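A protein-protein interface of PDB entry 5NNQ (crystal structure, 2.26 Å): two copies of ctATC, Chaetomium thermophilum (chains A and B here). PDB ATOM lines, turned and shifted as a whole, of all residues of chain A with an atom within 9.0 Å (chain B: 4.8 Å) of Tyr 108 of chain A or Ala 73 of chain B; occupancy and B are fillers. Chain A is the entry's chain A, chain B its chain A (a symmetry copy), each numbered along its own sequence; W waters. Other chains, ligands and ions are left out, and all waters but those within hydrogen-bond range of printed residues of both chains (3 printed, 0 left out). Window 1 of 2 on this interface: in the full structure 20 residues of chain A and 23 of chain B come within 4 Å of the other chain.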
ATOM      1  N   GLY A  53     -33.856  -3.996   1.926  1.00  0.00           N
ATOM      2  CA  GLY A  53     -32.605  -3.254   1.938  1.00  0.00           C
ATOM      3  C   GLY A  53     -32.211  -2.655   3.275  1.00  0.00           C
ATOM      4  O   GLY A  53     -31.132  -2.048   3.373  1.00  0.00           O
ATOM      5  N   LYS A  54     -33.052  -2.769   4.299  1.00  0.00           N
ATOM      6  CA  LYS A  54     -32.706  -2.286   5.626  1.00  0.00           C
ATOM      7  C   LYS A  54     -32.436  -3.457   6.574  1.00  0.00           C
ATOM      8  O   LYS A  54     -33.113  -4.489   6.528  1.00  0.00           O
ATOM      9  CB  LYS A  54     -33.818  -1.379   6.173  1.00  0.00           C
ATOM     10  CG  LYS A  54     -34.088  -0.128   5.285  1.00  0.00           C
ATOM     11  CD  LYS A  54     -32.891   0.819   5.277  1.00  0.00           C
ATOM     12  CE  LYS A  54     -33.099   2.006   4.336  1.00  0.00           C
ATOM     13  NZ  LYS A  54     -31.859   2.829   4.202  1.00  0.00           N
ATOM     14  N   VAL A  55     -31.462  -3.269   7.456  1.00  0.00           N
ATOM     15  CA  VAL A  55     -31.050  -4.274   8.427  1.00  0.00           C
ATOM     16  C   VAL A  55     -31.240  -3.698   9.828  1.00  0.00           C
ATOM     17  O   VAL A  55     -30.710  -2.623  10.139  1.00  0.00           O
ATOM     18  CB  VAL A  55     -29.587  -4.691   8.208  1.00  0.00           C
ATOM     19  CG1 VAL A  55     -29.162  -5.743   9.254  1.00  0.00           C
ATOM     20  CG2 VAL A  55     -29.367  -5.163   6.746  1.00  0.00           C
ATOM     21  N   LEU A  56     -32.002  -4.404  10.659  1.00  0.00           N
ATOM     22  CA  LEU A  56     -32.187  -4.066  12.060  1.00  0.00           C
ATOM     23  C   LEU A  56     -31.444  -5.082  12.910  1.00  0.00           C
ATOM     24  O   LEU A  56     -31.586  -6.299  12.711  1.00  0.00           O
ATOM     25  CB  LEU A  56     -33.660  -4.070  12.471  1.00  0.00           C
ATOM     26  CG  LEU A  56     -33.940  -3.834  13.980  1.00  0.00           C
ATOM     27  CD1 LEU A  56     -33.754  -2.342  14.339  1.00  0.00           C
ATOM     28  CD2 LEU A  56     -35.340  -4.199  14.364  1.00  0.00           C
ATOM     29  N   CYS A  57     -30.704  -4.594  13.885  1.00  0.00           N
ATOM     30  CA  CYS A  57     -30.038  -5.454  14.844  1.00  0.00           C
ATOM     31  C   CYS A  57     -30.690  -5.288  16.212  1.00  0.00           C
ATOM     32  O   CYS A  57     -30.854  -4.163  16.684  1.00  0.00           O
ATOM     33  CB  CYS A  57     -28.568  -5.099  14.899  1.00  0.00           C
ATOM     34  SG  CYS A  57     -27.846  -5.488  16.413  1.00  0.00           S
ATOM     35  N   ARG A  81     -34.328  -7.076   7.013  1.00  0.00           N
ATOM     36  CA  ARG A  81     -33.535  -8.162   7.569  1.00  0.00           C
ATOM     37  C   ARG A  81     -33.174  -7.834   9.013  1.00  0.00           C
ATOM     38  O   ARG A  81     -32.971  -6.665   9.367  1.00  0.00           O
ATOM     39  CB  ARG A  81     -32.249  -8.372   6.779  1.00  0.00           C
ATOM     40  CG  ARG A  81     -32.396  -8.643   5.279  1.00  0.00           C
ATOM     41  CD  ARG A  81     -33.300  -9.831   4.987  1.00  0.00           C
ATOM     42  NE  ARG A  81     -33.057 -10.386   3.659  1.00  0.00           N
ATOM     43  CZ  ARG A  81     -32.188 -11.366   3.386  1.00  0.00           C
ATOM     44  NH1 ARG A  81     -31.460 -11.927   4.358  1.00  0.00           N
ATOM     45  NH2 ARG A  81     -32.042 -11.804   2.130  1.00  0.00           N
ATOM     46  N   THR A  82     -33.104  -8.882   9.839  1.00  0.00           N
ATOM     47  CA  THR A  82     -32.800  -8.789  11.267  1.00  0.00           C
ATOM     48  C   THR A  82     -31.555  -9.602  11.636  1.00  0.00           C
ATOM     49  O   THR A  82     -31.310 -10.701  11.103  1.00  0.00           O
ATOM     50  CB  THR A  82     -33.967  -9.313  12.112  1.00  0.00           C
ATOM     51  OG1 THR A  82     -34.163 -10.703  11.789  1.00  0.00           O
ATOM     52  CG2 THR A  82     -35.244  -8.502  11.854  1.00  0.00           C
ATOM     53  N   ILE A  83     -30.797  -9.047  12.570  1.00  0.00           N
ATOM     54  CA  ILE A  83     -29.674  -9.706  13.232  1.00  0.00           C
ATOM     55  C   ILE A  83     -29.923  -9.671  14.744  1.00  0.00           C
ATOM     56  O   ILE A  83     -29.648  -8.668  15.416  1.00  0.00           O
ATOM     57  CB  ILE A  83     -28.339  -9.023  12.880  1.00  0.00           C
ATOM     58  CG1 ILE A  83     -28.141  -9.059  11.364  1.00  0.00           C
ATOM     59  CG2 ILE A  83     -27.170  -9.720  13.582  1.00  0.00           C
ATOM     60  CD1 ILE A  83     -26.973  -8.249  10.936  1.00  0.00           C
ATOM     61  N   PRO A  84     -30.473 -10.749  15.311  1.00  0.00           N
ATOM     62  CA  PRO A  84     -30.721 -10.823  16.765  1.00  0.00           C
ATOM     63  C   PRO A  84     -29.465 -11.232  17.519  1.00  0.00           C
ATOM     64  O   PRO A  84     -28.858 -12.258  17.231  1.00  0.00           O
ATOM     65  CB  PRO A  84     -31.818 -11.889  16.890  1.00  0.00           C
ATOM     66  CG  PRO A  84     -31.950 -12.570  15.535  1.00  0.00           C
ATOM     67  CD  PRO A  84     -30.952 -11.933  14.574  1.00  0.00           C
ATOM     68  N   ILE A  85     -29.074 -10.411  18.476  1.00  0.00           N
ATOM     69  CA  ILE A  85     -27.934 -10.653  19.352  1.00  0.00           C
ATOM     70  C   ILE A  85     -28.448 -10.888  20.789  1.00  0.00           C
ATOM     71  O   ILE A  85     -29.130 -10.014  21.391  1.00  0.00           O
ATOM     72  CB  ILE A  85     -26.955  -9.458  19.343  1.00  0.00           C
ATOM     73  CG1 ILE A  85     -26.663  -8.850  17.949  1.00  0.00           C
ATOM     74  CG2 ILE A  85     -25.682  -9.778  20.188  1.00  0.00           C
ATOM     75  CD1 ILE A  85     -25.671  -9.464  17.152  1.00  0.00           C
ATOM     76  N   ASP A 100     -18.608   0.281  22.958  1.00  0.00           N
ATOM     77  CA  ASP A 100     -17.869  -0.486  21.932  1.00  0.00           C
ATOM     78  C   ASP A 100     -18.784  -1.442  21.175  1.00  0.00           C
ATOM     79  O   ASP A 100     -18.669  -1.591  19.949  1.00  0.00           O
ATOM     80  CB  ASP A 100     -16.700  -1.291  22.546  1.00  0.00           C
ATOM     81  CG  ASP A 100     -15.487  -0.407  22.872  1.00  0.00           C
ATOM     82  OD1 ASP A 100     -15.664   0.844  22.895  1.00  0.00           O
ATOM     83  OD2 ASP A 100     -14.371  -0.963  23.119  1.00  0.00           O
ATOM     84  N   THR A 101     -19.706  -2.100  21.873  1.00  0.00           N
ATOM     85  CA  THR A 101     -20.606  -3.012  21.150  1.00  0.00           C
ATOM     86  C   THR A 101     -21.529  -2.243  20.206  1.00  0.00           C
ATOM     87  O   THR A 101     -21.733  -2.644  19.057  1.00  0.00           O
ATOM     88  CB  THR A 101     -21.414  -3.853  22.153  1.00  0.00           C
ATOM     89  OG1 THR A 101     -20.509  -4.676  22.924  1.00  0.00           O
ATOM     90  CG2 THR A 101     -22.413  -4.758  21.406  1.00  0.00           C
ATOM     91  N   LEU A 102     -22.082  -1.122  20.662  1.00  0.00           N
ATOM     92  CA  LEU A 102     -22.938  -0.315  19.796  1.00  0.00           C
ATOM     93  C   LEU A 102     -22.184   0.148  18.559  1.00  0.00           C
ATOM     94  O   LEU A 102     -22.671   0.020  17.423  1.00  0.00           O
ATOM     95  CB  LEU A 102     -23.462   0.888  20.582  1.00  0.00           C
ATOM     96  CG  LEU A 102     -24.527   0.557  21.615  1.00  0.00           C
ATOM     97  CD1 LEU A 102     -24.802   1.775  22.424  1.00  0.00           C
ATOM     98  CD2 LEU A 102     -25.780   0.054  20.894  1.00  0.00           C
ATOM     99  N   ARG A 103     -20.986   0.680  18.748  1.00  0.00           N
ATOM    100  CA  ARG A 103     -20.247   1.136  17.573  1.00  0.00           C
ATOM    101  C   ARG A 103     -19.852  -0.036  16.686  1.00  0.00           C
ATOM    102  O   ARG A 103     -19.894   0.076  15.465  1.00  0.00           O
ATOM    103  CB  ARG A 103     -19.063   1.976  18.042  1.00  0.00           C
ATOM    104  CG  ARG A 103     -19.508   3.474  18.480  1.00  0.00           C
ATOM    105  CD  ARG A 103     -18.385   4.210  19.189  1.00  0.00           C
ATOM    106  NE  ARG A 103     -17.959   3.545  20.415  1.00  0.00           N
ATOM    107  CZ  ARG A 103     -17.040   4.013  21.242  1.00  0.00           C
ATOM    108  NH1 ARG A 103     -16.458   5.191  21.000  1.00  0.00           N
ATOM    109  NH2 ARG A 103     -16.725   3.330  22.349  1.00  0.00           N
ATOM    110  N   THR A 104     -19.581  -1.213  17.266  1.00  0.00           N
ATOM    111  CA  THR A 104     -19.336  -2.384  16.428  1.00  0.00           C
ATOM    112  C   THR A 104     -20.515  -2.663  15.513  1.00  0.00           C
ATOM    113  O   THR A 104     -20.356  -2.791  14.286  1.00  0.00           O
ATOM    114  CB  THR A 104     -19.066  -3.587  17.304  1.00  0.00           C
ATOM    115  OG1 THR A 104     -17.823  -3.376  17.999  1.00  0.00           O
ATOM    116  CG2 THR A 104     -19.044  -4.863  16.438  1.00  0.00           C
ATOM    117  N   LEU A 105     -21.707  -2.791  16.111  1.00  0.00           N
ATOM    118  CA  LEU A 105     -22.910  -3.238  15.417  1.00  0.00           C
ATOM    119  C   LEU A 105     -23.516  -2.175  14.491  1.00  0.00           C
ATOM    120  O   LEU A 105     -24.175  -2.508  13.482  1.00  0.00           O
ATOM    121  CB  LEU A 105     -23.932  -3.663  16.474  1.00  0.00           C
ATOM    122  CG  LEU A 105     -23.550  -4.928  17.269  1.00  0.00           C
ATOM    123  CD1 LEU A 105     -24.692  -5.232  18.216  1.00  0.00           C
ATOM    124  CD2 LEU A 105     -23.293  -6.150  16.349  1.00  0.00           C
ATOM    125  N   ALA A 106     -23.311  -0.899  14.821  1.00  0.00           N
ATOM    126  CA  ALA A 106     -23.723   0.176  13.930  1.00  0.00           C
ATOM    127  C   ALA A 106     -23.116   0.042  12.536  1.00  0.00           C
ATOM    128  O   ALA A 106     -23.748   0.443  11.563  1.00  0.00           O
ATOM    129  CB  ALA A 106     -23.366   1.515  14.568  1.00  0.00           C
ATOM    130  N   ASN A 107     -21.923  -0.554  12.403  1.00  0.00           N
ATOM    131  CA  ASN A 107     -21.360  -0.806  11.064  1.00  0.00           C
ATOM    132  C   ASN A 107     -22.071  -1.896  10.268  1.00  0.00           C
ATOM    133  O   ASN A 107     -21.751  -2.077   9.079  1.00  0.00           O
ATOM    134  CB  ASN A 107     -19.880  -1.228  11.143  1.00  0.00           C
ATOM    135  CG  ASN A 107     -19.010  -0.146  11.706  1.00  0.00           C
ATOM    136  OD1 ASN A 107     -18.841   0.901  11.089  1.00  0.00           O
ATOM    137  ND2 ASN A 107     -18.468  -0.377  12.886  1.00  0.00           N
ATOM    138  N   TYR A 108     -22.976  -2.656  10.883  1.00  0.00           N
ATOM    139  CA  TYR A 108     -23.641  -3.747  10.182  1.00  0.00           C
ATOM    140  C   TYR A 108     -25.091  -3.464   9.880  1.00  0.00           C
ATOM    141  O   TYR A 108     -25.636  -4.023   8.937  1.00  0.00           O
ATOM    142  CB  TYR A 108     -23.571  -5.040  11.022  1.00  0.00           C
ATOM    143  CG  TYR A 108     -22.179  -5.413  11.433  1.00  0.00           C
ATOM    144  CD1 TYR A 108     -21.079  -5.076  10.635  1.00  0.00           C
ATOM    145  CD2 TYR A 108     -21.942  -6.030  12.641  1.00  0.00           C
ATOM    146  CE1 TYR A 108     -19.819  -5.369  11.028  1.00  0.00           C
ATOM    147  CE2 TYR A 108     -20.653  -6.350  13.029  1.00  0.00           C
ATOM    148  CZ  TYR A 108     -19.604  -6.048  12.203  1.00  0.00           C
ATOM    149  OH  TYR A 108     -18.313  -6.322  12.613  1.00  0.00           O
ATOM    150  N   SER A 109     -25.735  -2.645  10.684  1.00  0.00           N
ATOM    151  CA  SER A 109     -27.171  -2.467  10.596  1.00  0.00           C
ATOM    152  C   SER A 109     -27.502  -0.979  10.478  1.00  0.00           C
ATOM    153  O   SER A 109     -26.695  -0.087  10.784  1.00  0.00           O
ATOM    154  CB  SER A 109     -27.846  -3.061  11.834  1.00  0.00           C
ATOM    155  OG  SER A 109     -27.209  -2.503  12.964  1.00  0.00           O
ATOM    156  N   ASP A 110     -28.726  -0.726  10.063  1.00  0.00           N
ATOM    157  CA  ASP A 110     -29.238   0.627   9.942  1.00  0.00           C
ATOM    158  C   ASP A 110     -29.905   1.120  11.215  1.00  0.00           C
ATOM    159  O   ASP A 110     -30.154   2.308  11.342  1.00  0.00           O
ATOM    160  CB  ASP A 110     -30.202   0.665   8.739  1.00  0.00           C
ATOM    161  CG  ASP A 110     -29.540   0.102   7.469  1.00  0.00           C
ATOM    162  OD1 ASP A 110     -28.400   0.528   7.145  1.00  0.00           O
ATOM    163  OD2 ASP A 110     -30.102  -0.812   6.838  1.00  0.00           O
ATOM    164  N   ALA A 111     -30.122   0.261  12.198  1.00  0.00           N
ATOM    165  CA  ALA A 111     -30.629   0.701  13.491  1.00  0.00           C
ATOM    166  C   ALA A 111     -30.506  -0.455  14.476  1.00  0.00           C
ATOM    167  O   ALA A 111     -30.383  -1.611  14.074  1.00  0.00           O
ATOM    168  CB  ALA A 111     -32.072   1.143  13.389  1.00  0.00           C
ATOM    169  N   ILE A 112     -30.629  -0.139  15.765  1.00  0.00           N
ATOM    170  CA  ILE A 112     -30.420  -1.113  16.823  1.00  0.00           C
ATOM    171  C   ILE A 112     -31.545  -0.918  17.809  1.00  0.00           C
ATOM    172  O   ILE A 112     -31.827   0.223  18.180  1.00  0.00           O
ATOM    173  CB  ILE A 112     -29.056  -0.902  17.508  1.00  0.00           C
ATOM    174  CG1 ILE A 112     -27.902  -1.050  16.496  1.00  0.00           C
ATOM    175  CG2 ILE A 112     -28.880  -1.854  18.678  1.00  0.00           C
ATOM    176  CD1 ILE A 112     -26.537  -0.440  16.994  1.00  0.00           C
ATOM    177  N   PRO A 130     -23.801   5.803  16.078  1.00  0.00           N
ATOM    178  CA  PRO A 130     -24.058   6.617  14.880  1.00  0.00           C
ATOM    179  C   PRO A 130     -25.237   6.147  14.060  1.00  0.00           C
ATOM    180  O   PRO A 130     -25.284   6.484  12.886  1.00  0.00           O
ATOM    181  CB  PRO A 130     -22.760   6.445  14.066  1.00  0.00           C
ATOM    182  CG  PRO A 130     -22.334   4.963  14.416  1.00  0.00           C
ATOM    183  CD  PRO A 130     -22.743   4.781  15.848  1.00  0.00           C
ATOM    184  N   VAL A 131     -26.113   5.297  14.601  1.00  0.00           N
ATOM    185  CA  VAL A 131     -27.353   4.915  13.920  1.00  0.00           C
ATOM    186  C   VAL A 131     -28.473   5.041  14.937  1.00  0.00           C
ATOM    187  O   VAL A 131     -28.217   5.054  16.151  1.00  0.00           O
ATOM    188  CB  VAL A 131     -27.303   3.482  13.341  1.00  0.00           C
ATOM    189  CG1 VAL A 131     -26.149   3.356  12.370  1.00  0.00           C
ATOM    190  CG2 VAL A 131     -27.242   2.394  14.468  1.00  0.00           C
ATOM    191  N   THR B  65     -19.391 -11.670  18.951  1.00  0.00           N
ATOM    192  CA  THR B  65     -20.400 -10.810  18.331  1.00  0.00           C
ATOM    193  C   THR B  65     -19.866 -10.066  17.105  1.00  0.00           C
ATOM    194  O   THR B  65     -20.554  -9.945  16.089  1.00  0.00           O
ATOM    195  CB  THR B  65     -20.908  -9.799  19.383  1.00  0.00           C
ATOM    196  OG1 THR B  65     -21.580 -10.480  20.453  1.00  0.00           O
ATOM    197  CG2 THR B  65     -21.902  -8.795  18.757  1.00  0.00           C
ATOM    198  N   ARG B  66     -18.671  -9.496  17.200  1.00  0.00           N
ATOM    199  CA  ARG B  66     -18.156  -8.732  16.075  1.00  0.00           C
ATOM    200  C   ARG B  66     -18.016  -9.600  14.844  1.00  0.00           C
ATOM    201  O   ARG B  66     -18.448  -9.222  13.741  1.00  0.00           O
ATOM    202  CB  ARG B  66     -16.835  -8.082  16.471  1.00  0.00           C
ATOM    203  CG  ARG B  66     -15.546  -8.490  15.741  1.00  0.00           C
ATOM    204  CD  ARG B  66     -14.354  -8.005  16.613  1.00  0.00           C
ATOM    205  NE  ARG B  66     -14.872  -6.820  17.274  1.00  0.00           N
ATOM    206  CZ  ARG B  66     -15.086  -6.675  18.573  1.00  0.00           C
ATOM    207  NH1 ARG B  66     -14.725  -7.629  19.429  1.00  0.00           N
ATOM    208  NH2 ARG B  66     -15.658  -5.540  19.003  1.00  0.00           N
ATOM    209  N   ALA B  69     -21.834 -11.508  13.953  1.00  0.00           N
ATOM    210  CA  ALA B  69     -22.787 -10.585  13.361  1.00  0.00           C
ATOM    211  C   ALA B  69     -22.252  -9.992  12.050  1.00  0.00           C
ATOM    212  O   ALA B  69     -23.039  -9.707  11.141  1.00  0.00           O
ATOM    213  CB  ALA B  69     -23.094  -9.476  14.342  1.00  0.00           C
ATOM    214  N   SER B  70     -20.934  -9.767  11.944  1.00  0.00           N
ATOM    215  CA  SER B  70     -20.370  -9.350  10.651  1.00  0.00           C
ATOM    216  C   SER B  70     -20.698 -10.339   9.538  1.00  0.00           C
ATOM    217  O   SER B  70     -21.120  -9.944   8.439  1.00  0.00           O
ATOM    218  CB  SER B  70     -18.844  -9.214  10.752  1.00  0.00           C
ATOM    219  OG  SER B  70     -18.318  -8.822   9.500  1.00  0.00           O
ATOM    220  N   PHE B  71     -20.480 -11.643   9.777  1.00  0.00           N
ATOM    221  CA  PHE B  71     -20.857 -12.606   8.729  1.00  0.00           C
ATOM    222  C   PHE B  71     -22.359 -12.697   8.517  1.00  0.00           C
ATOM    223  O   PHE B  71     -22.816 -12.947   7.382  1.00  0.00           O
ATOM    224  CB  PHE B  71     -20.329 -13.987   9.026  1.00  0.00           C
ATOM    225  CG  PHE B  71     -18.856 -14.171   8.737  1.00  0.00           C
ATOM    226  CD1 PHE B  71     -18.398 -14.356   7.434  1.00  0.00           C
ATOM    227  CD2 PHE B  71     -17.942 -14.189   9.762  1.00  0.00           C
ATOM    228  CE1 PHE B  71     -17.038 -14.563   7.188  1.00  0.00           C
ATOM    229  CE2 PHE B  71     -16.556 -14.404   9.532  1.00  0.00           C
ATOM    230  CZ  PHE B  71     -16.122 -14.596   8.244  1.00  0.00           C
ATOM    231  N   ASP B  72     -23.154 -12.560   9.572  1.00  0.00           N
ATOM    232  CA  ASP B  72     -24.610 -12.603   9.392  1.00  0.00           C
ATOM    233  C   ASP B  72     -25.025 -11.473   8.468  1.00  0.00           C
ATOM    234  O   ASP B  72     -25.667 -11.690   7.436  1.00  0.00           O
ATOM    235  CB  ASP B  72     -25.323 -12.473  10.751  1.00  0.00           C
ATOM    236  CG  ASP B  72     -26.777 -12.835  10.686  1.00  0.00           C
ATOM    237  OD1 ASP B  72     -27.249 -13.055   9.557  1.00  0.00           O
ATOM    238  OD2 ASP B  72     -27.447 -12.923  11.752  1.00  0.00           O
ATOM    239  N   ALA B  73     -24.560 -10.265   8.786  1.00  0.00           N
ATOM    240  CA  ALA B  73     -24.936  -9.078   8.025  1.00  0.00           C
ATOM    241  C   ALA B  73     -24.366  -9.124   6.615  1.00  0.00           C
ATOM    242  O   ALA B  73     -25.061  -8.773   5.665  1.00  0.00           O
ATOM    243  CB  ALA B  73     -24.462  -7.820   8.745  1.00  0.00           C
ATOM    244  N   ALA B  74     -23.156  -9.660   6.439  1.00  0.00           N
ATOM    245  CA  ALA B  74     -22.645  -9.812   5.086  1.00  0.00           C
ATOM    246  C   ALA B  74     -23.521 -10.754   4.281  1.00  0.00           C
ATOM    247  O   ALA B  74     -24.004 -10.399   3.200  1.00  0.00           O
ATOM    248  CB  ALA B  74     -21.195 -10.294   5.104  1.00  0.00           C
ATOM    249  N   MET B  75     -23.776 -11.953   4.789  1.00  0.00           N
ATOM    250  CA  MET B  75     -24.611 -12.848   3.997  1.00  0.00           C
ATOM    251  C   MET B  75     -25.934 -12.185   3.642  1.00  0.00           C
ATOM    252  O   MET B  75     -26.369 -12.215   2.476  1.00  0.00           O
ATOM    253  CB  MET B  75     -24.880 -14.152   4.708  1.00  0.00           C
ATOM    254  CG  MET B  75     -25.632 -15.079   3.804  1.00  0.00           C
ATOM    255  SD  MET B  75     -24.519 -15.630   2.471  1.00  0.00           S
ATOM    256  CE  MET B  75     -25.500 -16.981   1.855  1.00  0.00           C
ATOM    257  N   GLN B  76     -26.605 -11.591   4.633  1.00  0.00           N
ATOM    258  CA  GLN B  76     -27.948 -11.098   4.358  1.00  0.00           C
ATOM    259  C   GLN B  76     -27.911  -9.922   3.379  1.00  0.00           C
ATOM    260  O   GLN B  76     -28.845  -9.728   2.592  1.00  0.00           O
ATOM    261  CB  GLN B  76     -28.659 -10.700   5.662  1.00  0.00           C
ATOM    262  CG  GLN B  76     -29.033 -11.920   6.515  1.00  0.00           C
ATOM    263  CD  GLN B  76     -30.064 -11.663   7.572  1.00  0.00           C
ATOM    264  OE1 GLN B  76     -31.251 -11.480   7.270  1.00  0.00           O
ATOM    265  NE2 GLN B  76     -29.635 -11.720   8.842  1.00  0.00           N
ATOM    266  N   ARG B  77     -26.863  -9.118   3.428  1.00  0.00           N
ATOM    267  CA  ARG B  77     -26.776  -8.002   2.514  1.00  0.00           C
ATOM    268  C   ARG B  77     -26.398  -8.447   1.103  1.00  0.00           C
ATOM    269  O   ARG B  77     -26.608  -7.682   0.165  1.00  0.00           O
ATOM    270  CB  ARG B  77     -25.790  -6.980   3.045  1.00  0.00           C
ATOM    271  CG  ARG B  77     -26.383  -6.007   4.074  1.00  0.00           C
ATOM    272  CD  ARG B  77     -25.365  -4.947   4.411  1.00  0.00           C
ATOM    273  NE  ARG B  77     -25.694  -4.092   5.568  1.00  0.00           N
ATOM    274  CZ  ARG B  77     -26.684  -3.202   5.591  1.00  0.00           C
ATOM    275  NH1 ARG B  77     -27.482  -3.059   4.553  1.00  0.00           N
ATOM    276  NH2 ARG B  77     -26.886  -2.460   6.660  1.00  0.00           N
ATOM    277  N   MET B 299     -14.273  -2.329  11.195  1.00  0.00           N
ATOM    278  CA  MET B 299     -15.328  -3.316  11.112  1.00  0.00           C
ATOM    279  C   MET B 299     -16.235  -3.076   9.914  1.00  0.00           C
ATOM    280  O   MET B 299     -16.764  -4.034   9.335  1.00  0.00           O
ATOM    281  CB  MET B 299     -16.065  -3.342  12.446  1.00  0.00           C
ATOM    282  CG  MET B 299     -15.240  -4.187  13.535  1.00  0.00           C
ATOM    283  SD  MET B 299     -15.624  -3.918  15.206  1.00  0.00           S
ATOM    284  CE  MET B 299     -15.842  -2.186  15.308  1.00  0.00           C
ATOM    285  N   LEU B 303     -16.981  -5.697   7.005  1.00  0.00           N
ATOM    286  CA  LEU B 303     -18.234  -6.004   6.331  1.00  0.00           C
ATOM    287  C   LEU B 303     -18.014  -6.178   4.827  1.00  0.00           C
ATOM    288  O   LEU B 303     -18.406  -7.205   4.244  1.00  0.00           O
ATOM    289  CB  LEU B 303     -19.267  -4.935   6.634  1.00  0.00           C
ATOM    290  CG  LEU B 303     -20.596  -5.205   5.934  1.00  0.00           C
ATOM    291  CD1 LEU B 303     -21.346  -6.372   6.578  1.00  0.00           C
ATOM    292  CD2 LEU B 303     -21.436  -3.935   5.932  1.00  0.00           C
HETATM  293  O   HOH W   1     -16.500  -6.670  10.404  1.00  0.00           O
HETATM  294  O   HOH W   2     -33.607 -11.759   8.396  1.00  0.00           O
HETATM  295  O   HOH W   3     -29.999 -13.588  11.851  1.00  0.00           O
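The backbone carbonyl oxygen (O) of Tyr 108 of chain A sits at hydrogen-bond distance from the guanidinium group (NH2) of Arg 77 of chain B (3.0 Å). The side-chain hydroxyl (OH) of Tyr 108 of chain A is in hydrogen-bond range of the backbone carbonyl oxygen (O) of Arg 66 of chain B (3.1 Å). NH2 of Arg 77 of chain B is in salt-bridge range of OD1 of Asp 110 of chain A, 3.4 Å away. NH1 of Arg 81 of chain A lies within hydrogen-bond range of OE1 of Gln 76 of chain B. The side-chain hydroxyl of Thr 104 of chain A lies close to the side-chain sulfur of Met 299 of chain B (3.6 Å). The guanidinium group (NH2) of Arg 66 of chain B sits at hydrogen-bond distance from the side-chain hydroxyl (OG1) of Thr 104 of chain A, at 3.2 Å. NE2 of Gln 76 of chain B is in hydrogen-bond range of O of Thr 82 of chain A (3.0 Å).
Printed residues of chain B within 4 Å of Arg 81 of chain A: Gln 76 (3.0 Å). Of the printed residues of chain B, Thr 82 of chain A touches Gln 76 (3.0 Å). Thr 101 of chain A touches none of the printed residues of chain B. Of the printed residues of chain B, Leu 105 of chain A touches Thr 65 and Ala 69. Of the printed residues of chain B, Tyr 108 of chain A touches Arg 66, Ser 70, Ala 73, Arg 77 and Met 299. Phe 71 of chain B touches none of the printed residues of chain A. Asp 72 of chain B touches just one residue of chain A: Ile 83 (3.7 Å). Of chain A, only Ile 83 (3.4 Å) and Tyr 108 (3.7 Å) come within 4 Å of Ala 73 of chain B. No residue of chain A comes within 4 Å of Ala 74 of chain B. The nearest residue of chain A that does not touch Ala 73 of chain B is Val 55 of chain A (5.2 Å). The nearest printed residue of chain A that does not touch Thr 65 of chain B is Ile 85 of chain A (4.2 Å).
Of the 25 printed residues of chain A, 12 touch a printed residue of chain B. Hydrophobic or aromatic side chains of chain A that line the printed part of chain B: Val 55, Ile 83, Ile 85, Leu 105 and Tyr 108. Along chain A the printed residues that touch a printed residue of chain B span positions 53 to 110. Of the 13 printed residues of chain B, 10 touch a printed residue of chain A. Printed residues of chain B that touch a printed residue of chain A: Thr 65, Arg 66, Ala 69, Ser 70, Asp 72, Ala 73, Gln 76, Arg 77, Met 299 and Leu 303. Hydrophobic or aromatic side chains of chain B within 4 Å of the printed part of chain A: Ala 69, Ala 73, Met 299 and Leu 303. Among the printed residues, 21 pairs touch across the chains. Among the printed residues, Asp or Glu carboxylates within 4 Å of a Lys or Arg side-chain nitrogen of the other chain: Asp 110 of chain A with Arg 77 of chain B.
Water W2 lies within hydrogen-bond range of OE1 of Gln 76 of chain B (2.6 Å) and N of Thr 82 of chain A (3.3 Å). Water W3 bridges the side-chain carboxylate of Asp 72 of chain B and the backbone carbonyl oxygen of Thr 82 of chain A. Water W1 lies within hydrogen-bond range of O of Met 299 of chain B (2.9 Å), OH of Tyr 108 of chain A (2.9 Å) and OG of Ser 70 of chain B (3.0 Å).
CG2 of Val 55 of chain A touches CZ of Arg 77 of chain B (3.5 Å). CG2 of Ile 83 of chain A touches OD2 of Asp 72 of chain B, 3.7 Å away. Ile 83 of chain A touches Gln 76 of chain B. Leu 105 of chain A touches Thr 65 of chain B (CD2 to CG2, 3.8 Å). CD2 of Leu 303 of chain B touches O of Asn 107 of chain A, 3.7 Å away. Ala 73 of chain B touches Tyr 108 of chain A (CB to CB, 3.7 Å). Tyr 108 of chain A touches Met 299 of chain B. Ser 109 of chain A touches Arg 77 of chain B.
The side-chain sulfur of Met 299 of chain B is in hydrogen-bond range of the guanidinium group of Arg 66 of chain B. ND2 of Asn 107 of chain A lies within hydrogen-bond range of O of Arg 103 of chain A. O of Lys 54 of chain A is in hydrogen-bond range of N of Arg 81 of chain A. OD1 of Asp 72 of chain B lies within hydrogen-bond range of NE2 of Gln 76 of chain B, 2.8 Å away. The side-chain hydroxyl of Ser 109 of chain A lies within hydrogen-bond range of the backbone carbonyl oxygen of Ala 111 of chain A (3.5 Å).
No position is printed for both chains.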
